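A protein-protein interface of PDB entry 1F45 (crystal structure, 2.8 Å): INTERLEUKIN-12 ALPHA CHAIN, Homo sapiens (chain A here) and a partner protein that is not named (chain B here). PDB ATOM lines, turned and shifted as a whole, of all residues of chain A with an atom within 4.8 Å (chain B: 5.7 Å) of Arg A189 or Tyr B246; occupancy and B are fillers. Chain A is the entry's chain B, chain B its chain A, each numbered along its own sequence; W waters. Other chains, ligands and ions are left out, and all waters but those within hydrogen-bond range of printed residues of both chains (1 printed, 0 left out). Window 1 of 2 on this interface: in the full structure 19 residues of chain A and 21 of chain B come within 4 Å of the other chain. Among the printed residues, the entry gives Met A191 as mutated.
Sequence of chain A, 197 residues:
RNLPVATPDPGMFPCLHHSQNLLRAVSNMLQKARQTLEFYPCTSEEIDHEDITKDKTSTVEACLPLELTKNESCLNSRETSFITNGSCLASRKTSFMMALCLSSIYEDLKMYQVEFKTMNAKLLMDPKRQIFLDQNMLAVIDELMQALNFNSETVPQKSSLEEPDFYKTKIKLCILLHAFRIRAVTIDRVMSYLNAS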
ATOM      1  N   VAL A  60     -20.721   2.153  18.249  1.00  0.00           N
ATOM      2  CA  VAL A  60     -19.901   3.113  18.963  1.00  0.00           C
ATOM      3  C   VAL A  60     -18.531   2.584  19.326  1.00  0.00           C
ATOM      4  O   VAL A  60     -17.555   3.318  19.266  1.00  0.00           O
ATOM      5  CB  VAL A  60     -20.545   3.572  20.306  1.00  0.00           C
ATOM      6  CG1 VAL A  60     -19.550   4.353  21.091  1.00  0.00           C
ATOM      7  CG2 VAL A  60     -21.710   4.400  20.060  1.00  0.00           C
ATOM      8  N   CYS A  63     -16.317   1.174  16.352  1.00  0.00           N
ATOM      9  CA  CYS A  63     -15.719   2.263  15.609  1.00  0.00           C
ATOM     10  C   CYS A  63     -15.173   3.249  16.584  1.00  0.00           C
ATOM     11  O   CYS A  63     -15.203   4.434  16.309  1.00  0.00           O
ATOM     12  CB  CYS A  63     -16.743   3.004  14.785  1.00  0.00           C
ATOM     13  SG  CYS A  63     -17.711   1.999  13.647  1.00  0.00           S
ATOM     14  N   PRO A  65     -12.581   5.568  18.303  1.00  0.00           N
ATOM     15  CA  PRO A  65     -11.311   6.161  17.862  1.00  0.00           C
ATOM     16  C   PRO A  65     -10.150   5.675  18.701  1.00  0.00           C
ATOM     17  O   PRO A  65     -10.312   5.500  19.891  1.00  0.00           O
ATOM     18  CB  PRO A  65     -11.558   7.667  18.031  1.00  0.00           C
ATOM     19  CG  PRO A  65     -13.006   7.750  17.745  1.00  0.00           C
ATOM     20  CD  PRO A  65     -13.589   6.611  18.532  1.00  0.00           C
ATOM     21  N   LEU A  68      -9.520   7.448  22.009  1.00  0.00           N
ATOM     22  CA  LEU A  68     -10.441   7.266  23.155  1.00  0.00           C
ATOM     23  C   LEU A  68     -10.161   5.991  23.973  1.00  0.00           C
ATOM     24  O   LEU A  68     -10.794   5.714  25.000  1.00  0.00           O
ATOM     25  CB  LEU A  68     -11.926   7.284  22.690  1.00  0.00           C
ATOM     26  CG  LEU A  68     -12.481   8.693  22.367  1.00  0.00           C
ATOM     27  CD1 LEU A  68     -13.966   8.600  22.151  1.00  0.00           C
ATOM     28  CD2 LEU A  68     -12.198   9.690  23.494  1.00  0.00           C
ATOM     29  N   ALA A 184     -27.334   8.237  13.333  1.00  0.00           N
ATOM     30  CA  ALA A 184     -26.700   8.822  12.133  1.00  0.00           C
ATOM     31  C   ALA A 184     -25.586   9.716  12.672  1.00  0.00           C
ATOM     32  O   ALA A 184     -24.503   9.777  12.103  1.00  0.00           O
ATOM     33  CB  ALA A 184     -27.706   9.668  11.298  1.00  0.00           C
ATOM     34  N   VAL A 185     -25.848  10.383  13.800  1.00  0.00           N
ATOM     35  CA  VAL A 185     -24.826  11.234  14.381  1.00  0.00           C
ATOM     36  C   VAL A 185     -23.532  10.473  14.599  1.00  0.00           C
ATOM     37  O   VAL A 185     -22.485  10.909  14.132  1.00  0.00           O
ATOM     38  CB  VAL A 185     -25.243  11.861  15.707  1.00  0.00           C
ATOM     39  CG1 VAL A 185     -24.001  12.375  16.433  1.00  0.00           C
ATOM     40  CG2 VAL A 185     -26.184  12.992  15.455  1.00  0.00           C
ATOM     41  N   THR A 186     -23.612   9.361  15.324  1.00  0.00           N
ATOM     42  CA  THR A 186     -22.444   8.540  15.546  1.00  0.00           C
ATOM     43  C   THR A 186     -21.747   8.221  14.198  1.00  0.00           C
ATOM     44  O   THR A 186     -20.542   8.479  14.032  1.00  0.00           O
ATOM     45  CB  THR A 186     -22.847   7.237  16.268  1.00  0.00           C
ATOM     46  OG1 THR A 186     -23.313   7.579  17.569  1.00  0.00           O
ATOM     47  CG2 THR A 186     -21.659   6.284  16.418  1.00  0.00           C
ATOM     48  N   ILE A 187     -22.509   7.659  13.253  1.00  0.00           N
ATOM     49  CA  ILE A 187     -22.022   7.287  11.935  1.00  0.00           C
ATOM     50  C   ILE A 187     -21.346   8.509  11.404  1.00  0.00           C
ATOM     51  O   ILE A 187     -20.190   8.450  11.014  1.00  0.00           O
ATOM     52  CB  ILE A 187     -23.211   6.883  11.049  1.00  0.00           C
ATOM     53  CG1 ILE A 187     -23.838   5.576  11.590  1.00  0.00           C
ATOM     54  CG2 ILE A 187     -22.834   6.806   9.583  1.00  0.00           C
ATOM     55  CD1 ILE A 187     -24.848   4.986  10.557  1.00  0.00           C
ATOM     56  N   ASP A 188     -22.021   9.652  11.464  1.00  0.00           N
ATOM     57  CA  ASP A 188     -21.391  10.870  10.968  1.00  0.00           C
ATOM     58  C   ASP A 188     -20.092  11.230  11.679  1.00  0.00           C
ATOM     59  O   ASP A 188     -19.187  11.782  11.091  1.00  0.00           O
ATOM     60  CB  ASP A 188     -22.358  12.056  11.024  1.00  0.00           C
ATOM     61  CG  ASP A 188     -21.889  13.246  10.157  1.00  0.00           C
ATOM     62  OD1 ASP A 188     -21.555  13.083   8.964  1.00  0.00           O
ATOM     63  OD2 ASP A 188     -21.856  14.365  10.683  1.00  0.00           O
ATOM     64  N   ARG A 189     -19.998  10.950  12.953  1.00  0.00           N
ATOM     65  CA  ARG A 189     -18.771  11.251  13.643  1.00  0.00           C
ATOM     66  C   ARG A 189     -17.667  10.334  13.111  1.00  0.00           C
ATOM     67  O   ARG A 189     -16.569  10.817  12.834  1.00  0.00           O
ATOM     68  CB  ARG A 189     -18.890  11.017  15.157  1.00  0.00           C
ATOM     69  CG  ARG A 189     -19.851  11.938  15.913  1.00  0.00           C
ATOM     70  CD  ARG A 189     -19.726  11.741  17.427  1.00  0.00           C
ATOM     71  NE  ARG A 189     -20.772  12.402  18.212  1.00  0.00           N
ATOM     72  CZ  ARG A 189     -20.779  13.689  18.579  1.00  0.00           C
ATOM     73  NH1 ARG A 189     -19.793  14.495  18.243  1.00  0.00           N
ATOM     74  NH2 ARG A 189     -21.782  14.180  19.288  1.00  0.00           N
ATOM     75  N   VAL A 190     -17.922   9.025  12.943  1.00  0.00           N
ATOM     76  CA  VAL A 190     -16.816   8.173  12.493  1.00  0.00           C
ATOM     77  C   VAL A 190     -16.488   8.528  11.077  1.00  0.00           C
ATOM     78  O   VAL A 190     -15.324   8.587  10.673  1.00  0.00           O
ATOM     79  CB  VAL A 190     -17.060   6.587  12.688  1.00  0.00           C
ATOM     80  CG1 VAL A 190     -18.170   6.325  13.731  1.00  0.00           C
ATOM     81  CG2 VAL A 190     -17.309   5.881  11.361  1.00  0.00           C
ATOM     82  N   MET A 191     -17.502   8.814  10.305  1.00  0.00           N
ATOM     83  CA  MET A 191     -17.166   9.186   8.965  1.00  0.00           C
ATOM     84  C   MET A 191     -16.264  10.430   8.943  1.00  0.00           C
ATOM     85  O   MET A 191     -15.322  10.499   8.173  1.00  0.00           O
ATOM     86  CB  MET A 191     -18.413   9.412   8.191  1.00  0.00           C
ATOM     87  CG  MET A 191     -19.055   8.124   7.801  1.00  0.00           C
ATOM     88  SD  MET A 191     -20.035   8.460   6.320  1.00  0.00           S
ATOM     89  CE  MET A 191     -20.961   9.897   6.804  1.00  0.00           C
ATOM     90  N   SER A 192     -16.527  11.403   9.808  1.00  0.00           N
ATOM     91  CA  SER A 192     -15.737  12.625   9.848  1.00  0.00           C
ATOM     92  C   SER A 192     -14.360  12.400  10.442  1.00  0.00           C
ATOM     93  O   SER A 192     -13.412  13.065  10.074  1.00  0.00           O
ATOM     94  CB  SER A 192     -16.512  13.734  10.614  1.00  0.00           C
ATOM     95  OG  SER A 192     -15.676  14.582  11.427  1.00  0.00           O
ATOM     96  N   TYR A 193     -14.240  11.473  11.363  1.00  0.00           N
ATOM     97  CA  TYR A 193     -12.945  11.207  11.943  1.00  0.00           C
ATOM     98  C   TYR A 193     -12.121  10.543  10.822  1.00  0.00           C
ATOM     99  O   TYR A 193     -10.964  10.892  10.582  1.00  0.00           O
ATOM    100  CB  TYR A 193     -13.151  10.299  13.135  1.00  0.00           C
ATOM    101  CG  TYR A 193     -11.948   9.593  13.695  1.00  0.00           C
ATOM    102  CD1 TYR A 193     -11.114  10.212  14.643  1.00  0.00           C
ATOM    103  CD2 TYR A 193     -11.696   8.255  13.353  1.00  0.00           C
ATOM    104  CE1 TYR A 193     -10.038   9.500  15.247  1.00  0.00           C
ATOM    105  CE2 TYR A 193     -10.661   7.541  13.934  1.00  0.00           C
ATOM    106  CZ  TYR A 193      -9.822   8.162  14.877  1.00  0.00           C
ATOM    107  OH  TYR A 193      -8.751   7.451  15.384  1.00  0.00           O
ATOM    108  N   TYR B 114     -18.177  16.663  26.138  1.00  0.00           N
ATOM    109  CA  TYR B 114     -18.809  15.407  26.468  1.00  0.00           C
ATOM    110  C   TYR B 114     -18.077  14.685  27.582  1.00  0.00           C
ATOM    111  O   TYR B 114     -18.185  13.456  27.696  1.00  0.00           O
ATOM    112  CB  TYR B 114     -18.828  14.489  25.269  1.00  0.00           C
ATOM    113  CG  TYR B 114     -19.640  15.007  24.115  1.00  0.00           C
ATOM    114  CD1 TYR B 114     -19.083  15.875  23.188  1.00  0.00           C
ATOM    115  CD2 TYR B 114     -20.956  14.666  23.968  1.00  0.00           C
ATOM    116  CE1 TYR B 114     -19.808  16.380  22.142  1.00  0.00           C
ATOM    117  CE2 TYR B 114     -21.694  15.182  22.932  1.00  0.00           C
ATOM    118  CZ  TYR B 114     -21.104  16.032  22.009  1.00  0.00           C
ATOM    119  OH  TYR B 114     -21.804  16.478  20.905  1.00  0.00           O
ATOM    120  N   PRO B 178     -16.913   9.743  26.734  1.00  0.00           N
ATOM    121  CA  PRO B 178     -17.401  10.856  25.917  1.00  0.00           C
ATOM    122  C   PRO B 178     -18.055  10.359  24.639  1.00  0.00           C
ATOM    123  O   PRO B 178     -18.908  11.049  24.114  1.00  0.00           O
ATOM    124  CB  PRO B 178     -16.135  11.630  25.602  1.00  0.00           C
ATOM    125  CG  PRO B 178     -15.145  11.180  26.639  1.00  0.00           C
ATOM    126  CD  PRO B 178     -15.445   9.734  26.764  1.00  0.00           C
ATOM    127  N   ALA B 179     -17.654   9.185  24.120  1.00  0.00           N
ATOM    128  CA  ALA B 179     -18.241   8.650  22.882  1.00  0.00           C
ATOM    129  C   ALA B 179     -19.538   7.875  23.010  1.00  0.00           C
ATOM    130  O   ALA B 179     -20.154   7.529  22.026  1.00  0.00           O
ATOM    131  CB  ALA B 179     -17.253   7.832  22.149  1.00  0.00           C
ATOM    132  N   PRO B 243     -10.995  13.046  20.259  1.00  0.00           N
ATOM    133  CA  PRO B 243     -10.461  13.657  19.036  1.00  0.00           C
ATOM    134  C   PRO B 243     -11.425  14.641  18.354  1.00  0.00           C
ATOM    135  O   PRO B 243     -12.564  14.311  18.077  1.00  0.00           O
ATOM    136  CB  PRO B 243     -10.122  12.435  18.170  1.00  0.00           C
ATOM    137  CG  PRO B 243     -11.110  11.421  18.615  1.00  0.00           C
ATOM    138  CD  PRO B 243     -11.166  11.586  20.105  1.00  0.00           C
ATOM    139  N   HIS B 244     -10.958  15.837  18.052  1.00  0.00           N
ATOM    140  CA  HIS B 244     -11.803  16.834  17.422  1.00  0.00           C
ATOM    141  C   HIS B 244     -12.590  16.407  16.206  1.00  0.00           C
ATOM    142  O   HIS B 244     -13.759  16.746  16.106  1.00  0.00           O
ATOM    143  CB  HIS B 244     -11.029  18.106  17.049  1.00  0.00           C
ATOM    144  CG  HIS B 244     -10.305  18.747  18.192  1.00  0.00           C
ATOM    145  ND1 HIS B 244     -10.703  18.610  19.510  1.00  0.00           N
ATOM    146  CD2 HIS B 244      -9.233  19.573  18.211  1.00  0.00           C
ATOM    147  CE1 HIS B 244      -9.908  19.328  20.289  1.00  0.00           C
ATOM    148  NE2 HIS B 244      -9.010  19.924  19.525  1.00  0.00           N
ATOM    149  N   SER B 245     -11.990  15.695  15.263  1.00  0.00           N
ATOM    150  CA  SER B 245     -12.736  15.294  14.059  1.00  0.00           C
ATOM    151  C   SER B 245     -13.944  14.412  14.440  1.00  0.00           C
ATOM    152  O   SER B 245     -14.930  14.326  13.692  1.00  0.00           O
ATOM    153  CB  SER B 245     -11.813  14.607  13.029  1.00  0.00           C
ATOM    154  OG  SER B 245     -11.140  13.478  13.582  1.00  0.00           O
ATOM    155  N   TYR B 246     -13.881  13.773  15.598  1.00  0.00           N
ATOM    156  CA  TYR B 246     -14.996  12.988  16.055  1.00  0.00           C
ATOM    157  C   TYR B 246     -16.008  13.945  16.737  1.00  0.00           C
ATOM    158  O   TYR B 246     -17.165  13.921  16.421  1.00  0.00           O
ATOM    159  CB  TYR B 246     -14.511  11.961  17.048  1.00  0.00           C
ATOM    160  CG  TYR B 246     -15.528  10.919  17.385  1.00  0.00           C
ATOM    161  CD1 TYR B 246     -15.638   9.798  16.596  1.00  0.00           C
ATOM    162  CD2 TYR B 246     -16.283  10.989  18.575  1.00  0.00           C
ATOM    163  CE1 TYR B 246     -16.442   8.731  16.955  1.00  0.00           C
ATOM    164  CE2 TYR B 246     -17.109   9.912  18.959  1.00  0.00           C
ATOM    165  CZ  TYR B 246     -17.164   8.772  18.124  1.00  0.00           C
ATOM    166  OH  TYR B 246     -17.858   7.645  18.462  1.00  0.00           O
ATOM    167  N   PHE B 247     -15.567  14.752  17.701  1.00  0.00           N
ATOM    168  CA  PHE B 247     -16.445  15.718  18.356  1.00  0.00           C
ATOM    169  C   PHE B 247     -16.312  17.086  17.652  1.00  0.00           C
ATOM    170  O   PHE B 247     -15.628  18.020  18.114  1.00  0.00           O
ATOM    171  CB  PHE B 247     -16.079  15.855  19.828  1.00  0.00           C
ATOM    172  CG  PHE B 247     -16.103  14.583  20.553  1.00  0.00           C
ATOM    173  CD1 PHE B 247     -14.933  13.907  20.815  1.00  0.00           C
ATOM    174  CD2 PHE B 247     -17.308  14.010  20.925  1.00  0.00           C
ATOM    175  CE1 PHE B 247     -14.943  12.662  21.441  1.00  0.00           C
ATOM    176  CE2 PHE B 247     -17.352  12.775  21.545  1.00  0.00           C
ATOM    177  CZ  PHE B 247     -16.152  12.090  21.807  1.00  0.00           C
ATOM    178  N   SER B 248     -16.974  17.185  16.515  1.00  0.00           N
ATOM    179  CA  SER B 248     -16.944  18.386  15.703  1.00  0.00           C
ATOM    180  C   SER B 248     -17.709  19.531  16.277  1.00  0.00           C
ATOM    181  O   SER B 248     -18.789  19.359  16.825  1.00  0.00           O
ATOM    182  CB  SER B 248     -17.568  18.125  14.330  1.00  0.00           C
ATOM    183  OG  SER B 248     -16.818  17.208  13.589  1.00  0.00           O
ATOM    184  N   ASP B 290     -21.767  23.008  19.260  1.00  0.00           N
ATOM    185  CA  ASP B 290     -21.676  21.551  18.986  1.00  0.00           C
ATOM    186  C   ASP B 290     -22.240  21.385  17.568  1.00  0.00           C
ATOM    187  O   ASP B 290     -23.133  22.137  17.157  1.00  0.00           O
ATOM    188  CB  ASP B 290     -22.509  20.707  19.949  1.00  0.00           C
ATOM    189  CG  ASP B 290     -22.405  19.225  19.655  1.00  0.00           C
ATOM    190  OD1 ASP B 290     -21.439  18.559  20.104  1.00  0.00           O
ATOM    191  OD2 ASP B 290     -23.302  18.736  18.948  1.00  0.00           O
ATOM    192  N   TYR B 292     -23.939  18.959  16.318  1.00  0.00           N
ATOM    193  CA  TYR B 292     -25.154  18.167  16.250  1.00  0.00           C
ATOM    194  C   TYR B 292     -26.373  18.369  17.125  1.00  0.00           C
ATOM    195  O   TYR B 292     -27.492  18.028  16.714  1.00  0.00           O
ATOM    196  CB  TYR B 292     -24.751  16.695  16.462  1.00  0.00           C
ATOM    197  CG  TYR B 292     -23.621  16.209  15.598  1.00  0.00           C
ATOM    198  CD1 TYR B 292     -22.318  16.075  16.105  1.00  0.00           C
ATOM    199  CD2 TYR B 292     -23.857  15.901  14.258  1.00  0.00           C
ATOM    200  CE1 TYR B 292     -21.265  15.644  15.281  1.00  0.00           C
ATOM    201  CE2 TYR B 292     -22.844  15.488  13.434  1.00  0.00           C
ATOM    202  CZ  TYR B 292     -21.557  15.365  13.930  1.00  0.00           C
ATOM    203  OH  TYR B 292     -20.587  15.037  13.013  1.00  0.00           O
ATOM    204  N   TYR B 293     -26.136  18.802  18.363  1.00  0.00           N
ATOM    205  CA  TYR B 293     -27.186  18.931  19.351  1.00  0.00           C
ATOM    206  C   TYR B 293     -27.369  20.311  19.891  1.00  0.00           C
ATOM    207  O   TYR B 293     -27.965  21.168  19.197  1.00  0.00           O
ATOM    208  CB  TYR B 293     -26.894  17.975  20.495  1.00  0.00           C
ATOM    209  CG  TYR B 293     -26.904  16.515  20.078  1.00  0.00           C
ATOM    210  CD1 TYR B 293     -28.078  15.890  19.683  1.00  0.00           C
ATOM    211  CD2 TYR B 293     -25.729  15.758  20.097  1.00  0.00           C
ATOM    212  CE1 TYR B 293     -28.084  14.556  19.328  1.00  0.00           C
ATOM    213  CE2 TYR B 293     -25.720  14.427  19.740  1.00  0.00           C
ATOM    214  CZ  TYR B 293     -26.891  13.825  19.359  1.00  0.00           C
ATOM    215  OH  TYR B 293     -26.880  12.499  19.008  1.00  0.00           O
HETATM  216  O   HOH W   1     -19.770  17.380  18.768  1.00  0.00           O
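Ala B179 touches Val A60. CB of Pro A65 touches CG of Pro B243 (3.8 Å). Pro A65 touches Tyr B246 (CG to CD1, 3.5 Å). Ala B179 touches Leu A68. Leu A68 touches Pro B243. Val A185 touches Tyr B292. CG2 of Val A185 touches OH of Tyr B293, at 3.7 Å. Arg A189 touches Phe B247 (NH1 to CA, 3.6 Å). CE2 of Tyr B293 touches NH2 of Arg A189, 3.97 Å away. Tyr A193 touches Ser B245.
Hydrophobic or aromatic side chains of chain A that line the printed part of chain B: Val A60, Pro A65, Leu A68, Val A185 and Tyr A193. Of the 12 printed residues of chain B, 9 touch a printed residue of chain A. Along chain B the printed residues that touch a printed residue of chain A span positions 114 to 293. Among the printed residues, no Asp or Glu carboxylate lies within 4 Å of a Lys or Arg side-chain nitrogen of the other chain.
Printed residues of chain B within 4 Å of Pro A65: Pro B243 and Tyr B246. Of the printed residues of chain B, Leu A68 touches Ala B179 and Pro B243. Printed residues of chain B within 4 Å of Val A185: Tyr B292 and Tyr B293. Of chain A, only Pro A65 (3.5 Å) and Arg A189 (3.2 Å) come within 4 Å of Tyr B246.
The side-chain carboxylate (OD2) of Asp B290 lies close to the side-chain hydroxyl (OH) of Tyr B114 (3.3 Å). OG of Ser B248 sits at hydrogen-bond distance from O of Ser B245, 3.4 Å away. OD2 of Asp B290 lies within hydrogen-bond range of N of Tyr B292 (2.7 Å). The backbone NH (N) of Tyr B293 is in hydrogen-bond range of the side-chain carboxylate (OD2) of Asp B290, 2.9 Å away.
The side-chain hydroxyl (OH) of Tyr B114 is in hydrogen-bond range of the guanidinium group (NH2) of Arg A189, 2.8 Å away. The guanidinium group (NH1) of Arg A189 is in hydrogen-bond range of the backbone carbonyl oxygen (O) of Tyr B246, 3.2 Å away. The side-chain hydroxyl of Tyr B292 sits at hydrogen-bond distance from the side-chain carboxylate of Asp A188, 2.7 Å away. O of Ser B245 lies close to OG of Ser A192, 2.4 Å away.
Water W1 lies within hydrogen-bond range of OD1 of Asp B290 (2.4 Å), NH1 of Arg A189 (2.9 Å), O of Ser B248 (2.9 Å) and OH of Tyr B114 (3.1 Å).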
